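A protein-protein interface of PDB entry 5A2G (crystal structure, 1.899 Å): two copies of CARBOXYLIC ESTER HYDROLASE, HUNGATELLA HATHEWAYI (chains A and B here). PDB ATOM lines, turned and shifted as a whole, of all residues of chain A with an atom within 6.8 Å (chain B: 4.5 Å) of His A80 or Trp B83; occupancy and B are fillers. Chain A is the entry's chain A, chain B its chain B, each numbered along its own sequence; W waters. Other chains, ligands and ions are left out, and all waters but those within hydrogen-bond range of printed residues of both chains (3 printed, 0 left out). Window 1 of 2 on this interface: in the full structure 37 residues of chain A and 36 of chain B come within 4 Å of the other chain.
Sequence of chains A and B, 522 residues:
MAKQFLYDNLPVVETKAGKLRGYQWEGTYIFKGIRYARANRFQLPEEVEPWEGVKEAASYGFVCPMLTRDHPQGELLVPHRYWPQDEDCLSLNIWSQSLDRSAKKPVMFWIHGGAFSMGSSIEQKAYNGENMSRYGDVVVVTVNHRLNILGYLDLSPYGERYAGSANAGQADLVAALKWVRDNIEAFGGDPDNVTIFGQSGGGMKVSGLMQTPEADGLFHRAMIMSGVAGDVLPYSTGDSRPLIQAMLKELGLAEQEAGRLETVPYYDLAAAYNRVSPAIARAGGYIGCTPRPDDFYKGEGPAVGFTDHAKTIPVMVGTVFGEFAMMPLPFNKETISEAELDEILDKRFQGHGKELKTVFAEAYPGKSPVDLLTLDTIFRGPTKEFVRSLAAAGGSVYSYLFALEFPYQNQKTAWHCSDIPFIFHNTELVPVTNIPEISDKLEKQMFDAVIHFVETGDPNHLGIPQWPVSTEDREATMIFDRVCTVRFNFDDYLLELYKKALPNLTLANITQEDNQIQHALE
N of Tyr A82 sits close to O of Tyr B82, 3.4 Å away.
The side-chain carboxylate of Glu A75 is in hydrogen-bond range of the backbone NH of His A80 (2.6 Å).
ND1 of His A80 sits at hydrogen-bond distance from O of Val A78 (3.0 Å).
The indole nitrogen of Trp B83 lies within hydrogen-bond range of the backbone carbonyl oxygen of Tyr B60 (3.0 Å).
NE1 of Trp B83 lies close to O of Gly B61 (3.2 Å).
The backbone NH of Val B63 sits at hydrogen-bond distance from the backbone carbonyl oxygen of Pro B84, 3.1 Å away.
Among the printed residues, merely in contact across the chains: Asp A70 with Phe B62 (3.4 Å), Asp A70 with Pro B84 (3.3 Å), Pro A72 with Trp B83 (3.4 Å), Pro A72 with Pro B84 (3.7 Å), Glu A75 with Trp B83 (3.6 Å), His A80 with Trp B83 (3.5 Å), Tyr A82 with Trp B83 (3.5 Å), Tyr A82 with Pro B84 (3.4 Å) and Trp A83 with Tyr B82 (3.5 Å).
Of the printed residues of chain B, His A80 touches Trp B83.
Trp B83 touches four residues of chain A.
Printed residues of chain B within 4 Å of Glu A75: Trp B83.
Printed residues of chain B within 4 Å of Tyr A82: Tyr B82 (3.4 Å), Trp B83 (3.5 Å) and Pro B84 (3.4 Å).
Glu A123 touches none of the printed residues of chain B.
The nearest printed residue of chain B that does not touch Tyr A82 is Ile B122 (7.1 Å).
Of the 18 printed residues of chain A, 6 touch a printed residue of chain B.
Printed residues of chain A that touch a printed residue of chain B: Asp A70, Pro A72, Glu A75, His A80, Tyr A82 and Trp A83.
Hydrophobic or aromatic side chains of chain A within 4 Å of the printed part of chain B: Pro A72, Tyr A82 and Trp A83.
Printed residues of chain B that touch a printed residue of chain A: Phe B62, Tyr B82, Trp B83 and Pro B84.
Hydrophobic or aromatic side chains of chain B that line the printed part of chain A: Phe B62, Tyr B82, Trp B83 and Pro B84.
Among the printed residues, no Asp or Glu carboxylate lies within 4 Å of a Lys or Arg side-chain nitrogen of the other chain.
Tyr B82 touches its own counterpart, Tyr A82.
Tyr A82 touches Trp B83, and with the chains exchanged Trp A83 touches Tyr B82.
3 positions are printed for both chains.
Of the 10 pairs that touch across the chains among the printed residues, 3 have their exchanged pair printed and touching as well.
Water W2 bridges O of Tyr B60 (2.6 Å) and O of Pro A72 (2.6 Å).
Water W3 bridges O of Tyr A82 (2.8 Å) and N of Tyr B82 (3.4 Å).
Water W1 bridges O of Tyr B82 (2.9 Å) and N of Tyr A82 (3.4 Å).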
ATOM      1  N   ASP A  70      28.845  -1.531 -22.538  1.00  0.00           N
ATOM      2  CA  ASP A  70      29.095  -0.916 -21.243  1.00  0.00           C
ATOM      3  C   ASP A  70      28.031  -1.331 -20.235  1.00  0.00           C
ATOM      4  O   ASP A  70      26.900  -1.653 -20.605  1.00  0.00           O
ATOM      5  CB  ASP A  70      29.140   0.610 -21.382  1.00  0.00           C
ATOM      6  CG  ASP A  70      30.216   1.076 -22.360  1.00  0.00           C
ATOM      7  OD1 ASP A  70      31.229   0.366 -22.518  1.00  0.00           O
ATOM      8  OD2 ASP A  70      30.057   2.146 -22.977  1.00  0.00           O
ATOM      9  N   PRO A  72      26.960   0.465 -16.878  1.00  0.00           N
ATOM     10  CA  PRO A  72      27.120   1.556 -15.906  1.00  0.00           C
ATOM     11  C   PRO A  72      26.338   1.336 -14.608  1.00  0.00           C
ATOM     12  O   PRO A  72      25.108   1.314 -14.615  1.00  0.00           O
ATOM     13  CB  PRO A  72      26.595   2.780 -16.667  1.00  0.00           C
ATOM     14  CG  PRO A  72      25.631   2.224 -17.661  1.00  0.00           C
ATOM     15  CD  PRO A  72      26.104   0.846 -18.018  1.00  0.00           C
ATOM     16  N   GLN A  73      27.054   1.185 -13.495  1.00  0.00           N
ATOM     17  CA  GLN A  73      26.412   0.881 -12.224  1.00  0.00           C
ATOM     18  C   GLN A  73      26.907   1.787 -11.104  1.00  0.00           C
ATOM     19  O   GLN A  73      26.651   1.538  -9.923  1.00  0.00           O
ATOM     20  CB  GLN A  73      26.636  -0.585 -11.862  1.00  0.00           C
ATOM     21  CG  GLN A  73      26.044  -1.545 -12.875  1.00  0.00           C
ATOM     22  CD  GLN A  73      26.106  -2.990 -12.426  1.00  0.00           C
ATOM     23  OE1 GLN A  73      25.121  -3.540 -11.930  1.00  0.00           O
ATOM     24  NE2 GLN A  73      27.258  -3.615 -12.605  1.00  0.00           N
ATOM     25  N   GLY A  74      27.611   2.844 -11.489  1.00  0.00           N
ATOM     26  CA  GLY A  74      28.141   3.808 -10.547  1.00  0.00           C
ATOM     27  C   GLY A  74      28.005   5.204 -11.114  1.00  0.00           C
ATOM     28  O   GLY A  74      28.955   5.986 -11.117  1.00  0.00           O
ATOM     29  N   GLU A  75      26.803   5.521 -11.591  1.00  0.00           N
ATOM     30  CA  GLU A  75      26.588   6.781 -12.288  1.00  0.00           C
ATOM     31  C   GLU A  75      26.638   7.997 -11.382  1.00  0.00           C
ATOM     32  O   GLU A  75      26.732   9.122 -11.868  1.00  0.00           O
ATOM     33  CB  GLU A  75      25.257   6.747 -13.037  1.00  0.00           C
ATOM     34  CG  GLU A  75      25.313   5.879 -14.263  1.00  0.00           C
ATOM     35  CD  GLU A  75      26.342   6.368 -15.254  1.00  0.00           C
ATOM     36  OE1 GLU A  75      26.126   7.443 -15.850  1.00  0.00           O
ATOM     37  OE2 GLU A  75      27.377   5.684 -15.427  1.00  0.00           O
ATOM     38  N   LEU A  77      29.105   8.426  -9.288  1.00  0.00           N
ATOM     39  CA  LEU A  77      30.544   8.723  -9.311  1.00  0.00           C
ATOM     40  C   LEU A  77      30.998   9.346 -10.627  1.00  0.00           C
ATOM     41  O   LEU A  77      31.822  10.260 -10.634  1.00  0.00           O
ATOM     42  CB  LEU A  77      31.356   7.454  -9.065  1.00  0.00           C
ATOM     43  CG  LEU A  77      31.086   6.710  -7.754  1.00  0.00           C
ATOM     44  CD1 LEU A  77      31.911   5.449  -7.675  1.00  0.00           C
ATOM     45  CD2 LEU A  77      31.372   7.602  -6.577  1.00  0.00           C
ATOM     46  N   VAL A  78      30.480   8.809 -11.734  1.00  0.00           N
ATOM     47  CA  VAL A  78      30.796   9.271 -13.088  1.00  0.00           C
ATOM     48  C   VAL A  78      29.552   9.207 -13.977  1.00  0.00           C
ATOM     49  O   VAL A  78      29.222   8.143 -14.506  1.00  0.00           O
ATOM     50  CB  VAL A  78      31.905   8.416 -13.752  1.00  0.00           C
ATOM     51  CG1 VAL A  78      32.264   8.982 -15.124  1.00  0.00           C
ATOM     52  CG2 VAL A  78      33.132   8.313 -12.863  1.00  0.00           C
ATOM     53  N   PRO A  79      28.842  10.337 -14.134  1.00  0.00           N
ATOM     54  CA  PRO A  79      27.668  10.356 -15.009  1.00  0.00           C
ATOM     55  C   PRO A  79      28.055  10.269 -16.493  1.00  0.00           C
ATOM     56  O   PRO A  79      28.821  11.105 -17.000  1.00  0.00           O
ATOM     57  CB  PRO A  79      27.005  11.701 -14.676  1.00  0.00           C
ATOM     58  CG  PRO A  79      27.588  12.098 -13.336  1.00  0.00           C
ATOM     59  CD  PRO A  79      28.996  11.609 -13.416  1.00  0.00           C
ATOM     60  N   HIS A  80      27.524   9.245 -17.162  1.00  0.00           N
ATOM     61  CA  HIS A  80      27.850   8.938 -18.557  1.00  0.00           C
ATOM     62  C   HIS A  80      26.755   9.288 -19.574  1.00  0.00           C
ATOM     63  O   HIS A  80      25.587   9.482 -19.222  1.00  0.00           O
ATOM     64  CB  HIS A  80      28.176   7.445 -18.708  1.00  0.00           C
ATOM     65  CG  HIS A  80      29.472   7.034 -18.083  1.00  0.00           C
ATOM     66  ND1 HIS A  80      29.537   6.351 -16.887  1.00  0.00           N
ATOM     67  CD2 HIS A  80      30.752   7.211 -18.486  1.00  0.00           C
ATOM     68  CE1 HIS A  80      30.800   6.124 -16.579  1.00  0.00           C
ATOM     69  NE2 HIS A  80      31.559   6.635 -17.532  1.00  0.00           N
ATOM     70  N   ARG A  81      27.167   9.343 -20.841  1.00  0.00           N
ATOM     71  CA  ARG A  81      26.275   9.478 -21.994  1.00  0.00           C
ATOM     72  C   ARG A  81      26.715   8.502 -23.077  1.00  0.00           C
ATOM     73  O   ARG A  81      27.903   8.197 -23.196  1.00  0.00           O
ATOM     74  CB  ARG A  81      26.292  10.897 -22.556  1.00  0.00           C
ATOM     75  CG  ARG A  81      25.696  11.950 -21.654  1.00  0.00           C
ATOM     76  CD  ARG A  81      25.757  13.303 -22.317  1.00  0.00           C
ATOM     77  NE  ARG A  81      27.126  13.825 -22.359  1.00  0.00           N
ATOM     78  CZ  ARG A  81      27.475  14.958 -22.963  1.00  0.00           C
ATOM     79  NH1 ARG A  81      26.557  15.686 -23.584  1.00  0.00           N
ATOM     80  NH2 ARG A  81      28.740  15.375 -22.941  1.00  0.00           N
ATOM     81  N   TYR A  82      25.766   8.009 -23.867  1.00  0.00           N
ATOM     82  CA  TYR A  82      26.092   7.084 -24.943  1.00  0.00           C
ATOM     83  C   TYR A  82      25.414   7.521 -26.243  1.00  0.00           C
ATOM     84  O   TYR A  82      24.572   8.427 -26.245  1.00  0.00           O
ATOM     85  CB  TYR A  82      25.703   5.660 -24.554  1.00  0.00           C
ATOM     86  CG  TYR A  82      26.378   5.257 -23.267  1.00  0.00           C
ATOM     87  CD1 TYR A  82      27.680   4.761 -23.264  1.00  0.00           C
ATOM     88  CD2 TYR A  82      25.738   5.421 -22.050  1.00  0.00           C
ATOM     89  CE1 TYR A  82      28.315   4.420 -22.068  1.00  0.00           C
ATOM     90  CE2 TYR A  82      26.364   5.085 -20.859  1.00  0.00           C
ATOM     91  CZ  TYR A  82      27.647   4.583 -20.875  1.00  0.00           C
ATOM     92  OH  TYR A  82      28.252   4.251 -19.681  1.00  0.00           O
ATOM     93  N   TRP A  83      25.799   6.887 -27.345  1.00  0.00           N
ATOM     94  CA  TRP A  83      25.456   7.391 -28.666  1.00  0.00           C
ATOM     95  C   TRP A  83      25.565   6.267 -29.711  1.00  0.00           C
ATOM     96  O   TRP A  83      26.316   5.312 -29.521  1.00  0.00           O
ATOM     97  CB  TRP A  83      26.373   8.582 -29.009  1.00  0.00           C
ATOM     98  CG  TRP A  83      25.804   9.553 -30.009  1.00  0.00           C
ATOM     99  CD1 TRP A  83      26.118   9.640 -31.332  1.00  0.00           C
ATOM    100  CD2 TRP A  83      24.823  10.570 -29.762  1.00  0.00           C
ATOM    101  NE1 TRP A  83      25.393  10.637 -31.927  1.00  0.00           N
ATOM    102  CE2 TRP A  83      24.590  11.226 -30.987  1.00  0.00           C
ATOM    103  CE3 TRP A  83      24.109  10.979 -28.631  1.00  0.00           C
ATOM    104  CZ2 TRP A  83      23.673  12.272 -31.117  1.00  0.00           C
ATOM    105  CZ3 TRP A  83      23.208  12.033 -28.756  1.00  0.00           C
ATOM    106  CH2 TRP A  83      22.998  12.662 -29.991  1.00  0.00           C
ATOM    107  N   ILE A 122      31.593  12.698 -25.884  1.00  0.00           N
ATOM    108  CA  ILE A 122      30.470  13.058 -25.033  1.00  0.00           C
ATOM    109  C   ILE A 122      30.214  12.002 -23.961  1.00  0.00           C
ATOM    110  O   ILE A 122      29.224  12.075 -23.232  1.00  0.00           O
ATOM    111  CB  ILE A 122      29.179  13.275 -25.862  1.00  0.00           C
ATOM    112  CG1 ILE A 122      28.731  11.970 -26.534  1.00  0.00           C
ATOM    113  CG2 ILE A 122      29.407  14.363 -26.906  1.00  0.00           C
ATOM    114  CD1 ILE A 122      27.339  12.049 -27.182  1.00  0.00           C
ATOM    115  N   GLU A 123      31.116  11.034 -23.848  1.00  0.00           N
ATOM    116  CA  GLU A 123      30.840   9.873 -23.007  1.00  0.00           C
ATOM    117  C   GLU A 123      30.636  10.216 -21.528  1.00  0.00           C
ATOM    118  O   GLU A 123      29.974   9.461 -20.808  1.00  0.00           O
ATOM    119  CB  GLU A 123      31.950   8.838 -23.153  1.00  0.00           C
ATOM    120  CG  GLU A 123      31.484   7.435 -22.819  1.00  0.00           C
ATOM    121  CD  GLU A 123      32.376   6.752 -21.805  1.00  0.00           C
ATOM    122  OE1 GLU A 123      33.181   7.453 -21.151  1.00  0.00           O
ATOM    123  OE2 GLU A 123      32.281   5.514 -21.673  1.00  0.00           O
ATOM    124  N   GLN A 124      31.180  11.345 -21.070  1.00  0.00           N
ATOM    125  CA  GLN A 124      30.856  11.826 -19.727  1.00  0.00           C
ATOM    126  C   GLN A 124      30.047  13.108 -19.844  1.00  0.00           C
ATOM    127  O   GLN A 124      30.321  13.933 -20.711  1.00  0.00           O
ATOM    128  CB  GLN A 124      32.117  12.048 -18.876  1.00  0.00           C
ATOM    129  CG  GLN A 124      32.794  10.745 -18.438  1.00  0.00           C
ATOM    130  CD  GLN A 124      33.922  10.937 -17.424  1.00  0.00           C
ATOM    131  OE1 GLN A 124      33.971  11.933 -16.697  1.00  0.00           O
ATOM    132  NE2 GLN A 124      34.825   9.963 -17.363  1.00  0.00           N
ATOM    133  N   LYS A 125      29.032  13.267 -18.992  1.00  0.00           N
ATOM    134  CA  LYS A 125      28.226  14.488 -19.013  1.00  0.00           C
ATOM    135  C   LYS A 125      29.137  15.692 -18.805  1.00  0.00           C
ATOM    136  O   LYS A 125      28.914  16.779 -19.354  1.00  0.00           O
ATOM    137  CB  LYS A 125      27.123  14.449 -17.947  1.00  0.00           C
ATOM    138  CG  LYS A 125      26.103  13.331 -18.129  1.00  0.00           C
ATOM    139  CD  LYS A 125      24.882  13.505 -17.217  1.00  0.00           C
ATOM    140  CE  LYS A 125      24.064  14.726 -17.619  1.00  0.00           C
ATOM    141  NZ  LYS A 125      22.794  14.856 -16.852  1.00  0.00           N
ATOM    142  N   TYR A 127      32.016  16.259 -19.915  1.00  0.00           N
ATOM    143  CA  TYR A 127      32.799  16.657 -21.092  1.00  0.00           C
ATOM    144  C   TYR A 127      32.171  17.832 -21.846  1.00  0.00           C
ATOM    145  O   TYR A 127      32.765  18.345 -22.796  1.00  0.00           O
ATOM    146  CB  TYR A 127      32.967  15.499 -22.092  1.00  0.00           C
ATOM    147  CG  TYR A 127      33.767  14.291 -21.647  1.00  0.00           C
ATOM    148  CD1 TYR A 127      34.479  14.279 -20.453  1.00  0.00           C
ATOM    149  CD2 TYR A 127      33.805  13.158 -22.441  1.00  0.00           C
ATOM    150  CE1 TYR A 127      35.207  13.155 -20.067  1.00  0.00           C
ATOM    151  CE2 TYR A 127      34.518  12.045 -22.074  1.00  0.00           C
ATOM    152  CZ  TYR A 127      35.218  12.040 -20.884  1.00  0.00           C
ATOM    153  OH  TYR A 127      35.913  10.906 -20.533  1.00  0.00           O
ATOM    154  N   CYS A 417      38.419   9.903 -12.142  1.00  0.00           N
ATOM    155  CA  CYS A 417      37.529  10.820 -12.899  1.00  0.00           C
ATOM    156  C   CYS A 417      36.805  11.857 -12.050  1.00  0.00           C
ATOM    157  O   CYS A 417      36.045  12.659 -12.592  1.00  0.00           O
ATOM    158  CB  CYS A 417      36.448  10.082 -13.706  1.00  0.00           C
ATOM    159  SG  CYS A 417      37.025   8.857 -14.847  1.00  0.00           S
ATOM    160  N   TYR B  60      20.758   4.734 -14.521  1.00  0.00           N
ATOM    161  CA  TYR B  60      19.774   4.322 -15.524  1.00  0.00           C
ATOM    162  C   TYR B  60      20.067   2.897 -15.962  1.00  0.00           C
ATOM    163  O   TYR B  60      21.215   2.555 -16.235  1.00  0.00           O
ATOM    164  CB  TYR B  60      19.786   5.258 -16.737  1.00  0.00           C
ATOM    165  CG  TYR B  60      19.187   6.616 -16.486  1.00  0.00           C
ATOM    166  CD1 TYR B  60      17.915   6.755 -15.942  1.00  0.00           C
ATOM    167  CD2 TYR B  60      19.896   7.773 -16.797  1.00  0.00           C
ATOM    168  CE1 TYR B  60      17.368   8.018 -15.712  1.00  0.00           C
ATOM    169  CE2 TYR B  60      19.360   9.024 -16.576  1.00  0.00           C
ATOM    170  CZ  TYR B  60      18.099   9.143 -16.034  1.00  0.00           C
ATOM    171  OH  TYR B  60      17.591  10.400 -15.814  1.00  0.00           O
ATOM    172  N   GLY B  61      19.035   2.065 -16.024  1.00  0.00           N
ATOM    173  CA  GLY B  61      19.228   0.670 -16.369  1.00  0.00           C
ATOM    174  C   GLY B  61      19.412   0.476 -17.859  1.00  0.00           C
ATOM    175  O   GLY B  61      19.315   1.435 -18.624  1.00  0.00           O
ATOM    176  N   PHE B  62      19.685  -0.762 -18.269  1.00  0.00           N
ATOM    177  CA  PHE B  62      19.794  -1.100 -19.682  1.00  0.00           C
ATOM    178  C   PHE B  62      18.515  -0.739 -20.438  1.00  0.00           C
ATOM    179  O   PHE B  62      17.416  -0.859 -19.898  1.00  0.00           O
ATOM    180  CB  PHE B  62      20.075  -2.594 -19.872  1.00  0.00           C
ATOM    181  CG  PHE B  62      21.463  -3.021 -19.484  1.00  0.00           C
ATOM    182  CD1 PHE B  62      22.577  -2.437 -20.068  1.00  0.00           C
ATOM    183  CD2 PHE B  62      21.656  -4.038 -18.557  1.00  0.00           C
ATOM    184  CE1 PHE B  62      23.861  -2.843 -19.717  1.00  0.00           C
ATOM    185  CE2 PHE B  62      22.934  -4.448 -18.207  1.00  0.00           C
ATOM    186  CZ  PHE B  62      24.034  -3.850 -18.788  1.00  0.00           C
ATOM    187  N   VAL B  63      18.660  -0.309 -21.688  1.00  0.00           N
ATOM    188  CA  VAL B  63      17.505  -0.093 -22.539  1.00  0.00           C
ATOM    189  C   VAL B  63      17.393  -1.251 -23.539  1.00  0.00           C
ATOM    190  O   VAL B  63      18.317  -2.055 -23.675  1.00  0.00           O
ATOM    191  CB  VAL B  63      17.584   1.262 -23.262  1.00  0.00           C
ATOM    192  CG1 VAL B  63      17.826   2.373 -22.244  1.00  0.00           C
ATOM    193  CG2 VAL B  63      18.666   1.243 -24.305  1.00  0.00           C
ATOM    194  N   TYR B  82      21.168   8.186 -25.538  1.00  0.00           N
ATOM    195  CA  TYR B  82      21.198   6.758 -25.819  1.00  0.00           C
ATOM    196  C   TYR B  82      21.935   6.043 -24.710  1.00  0.00           C
ATOM    197  O   TYR B  82      22.584   6.683 -23.873  1.00  0.00           O
ATOM    198  CB  TYR B  82      21.843   6.497 -27.178  1.00  0.00           C
ATOM    199  CG  TYR B  82      21.139   7.262 -28.262  1.00  0.00           C
ATOM    200  CD1 TYR B  82      20.031   6.727 -28.902  1.00  0.00           C
ATOM    201  CD2 TYR B  82      21.546   8.540 -28.609  1.00  0.00           C
ATOM    202  CE1 TYR B  82      19.367   7.435 -29.889  1.00  0.00           C
ATOM    203  CE2 TYR B  82      20.884   9.259 -29.587  1.00  0.00           C
ATOM    204  CZ  TYR B  82      19.796   8.698 -30.229  1.00  0.00           C
ATOM    205  OH  TYR B  82      19.131   9.412 -31.209  1.00  0.00           O
ATOM    206  N   TRP B  83      21.825   4.721 -24.690  1.00  0.00           N
ATOM    207  CA  TRP B  83      22.265   3.952 -23.531  1.00  0.00           C
ATOM    208  C   TRP B  83      22.532   2.510 -23.954  1.00  0.00           C
ATOM    209  O   TRP B  83      21.944   2.040 -24.929  1.00  0.00           O
ATOM    210  CB  TRP B  83      21.200   4.032 -22.429  1.00  0.00           C
ATOM    211  CG  TRP B  83      21.691   3.796 -21.020  1.00  0.00           C
ATOM    212  CD1 TRP B  83      21.588   2.646 -20.307  1.00  0.00           C
ATOM    213  CD2 TRP B  83      22.351   4.743 -20.165  1.00  0.00           C
ATOM    214  NE1 TRP B  83      22.140   2.809 -19.056  1.00  0.00           N
ATOM    215  CE2 TRP B  83      22.622   4.087 -18.949  1.00  0.00           C
ATOM    216  CE3 TRP B  83      22.744   6.074 -20.313  1.00  0.00           C
ATOM    217  CZ2 TRP B  83      23.265   4.719 -17.882  1.00  0.00           C
ATOM    218  CZ3 TRP B  83      23.389   6.703 -19.251  1.00  0.00           C
ATOM    219  CH2 TRP B  83      23.638   6.023 -18.052  1.00  0.00           C
ATOM    220  N   PRO B  84      23.444   1.816 -23.242  1.00  0.00           N
ATOM    221  CA  PRO B  84      23.734   0.406 -23.524  1.00  0.00           C
ATOM    222  C   PRO B  84      22.481  -0.457 -23.548  1.00  0.00           C
ATOM    223  O   PRO B  84      21.606  -0.318 -22.683  1.00  0.00           O
ATOM    224  CB  PRO B  84      24.657  -0.014 -22.368  1.00  0.00           C
ATOM    225  CG  PRO B  84      24.672   1.148 -21.401  1.00  0.00           C
ATOM    226  CD  PRO B  84      24.361   2.355 -22.224  1.00  0.00           C
ATOM    227  N   GLN B  85      22.425  -1.341 -24.540  1.00  0.00           N
ATOM    228  CA  GLN B  85      21.279  -2.203 -24.797  1.00  0.00           C
ATOM    229  C   GLN B  85      21.469  -3.606 -24.213  1.00  0.00           C
ATOM    230  O   GLN B  85      22.547  -4.190 -24.306  1.00  0.00           O
ATOM    231  CB  GLN B  85      21.033  -2.287 -26.314  1.00  0.00           C
ATOM    232  CG  GLN B  85      20.763  -0.930 -26.969  1.00  0.00           C
ATOM    233  CD  GLN B  85      20.944  -0.950 -28.477  1.00  0.00           C
ATOM    234  OE1 GLN B  85      20.522  -1.883 -29.154  1.00  0.00           O
ATOM    235  NE2 GLN B  85      21.584   0.085 -29.008  1.00  0.00           N
ATOM    236  N   ILE B 122      14.636   7.286 -21.316  1.00  0.00           N
ATOM    237  CA  ILE B 122      15.555   8.413 -21.320  1.00  0.00           C
ATOM    238  C   ILE B 122      15.898   8.873 -22.736  1.00  0.00           C
ATOM    239  O   ILE B 122      16.764   9.726 -22.914  1.00  0.00           O
ATOM    240  CB  ILE B 122      16.863   8.059 -20.572  1.00  0.00           C
ATOM    241  CG1 ILE B 122      17.566   6.860 -21.219  1.00  0.00           C
ATOM    242  CG2 ILE B 122      16.554   7.750 -19.106  1.00  0.00           C
ATOM    243  CD1 ILE B 122      18.914   6.513 -20.557  1.00  0.00           C
HETATM  244  O   HOH W   1      22.923   9.270 -22.571  1.00  0.00           O
HETATM  245  O   HOH W   2      22.614   0.696 -15.174  1.00  0.00           O
HETATM  246  O   HOH W   3      23.430  10.688 -24.951  1.00  0.00           O
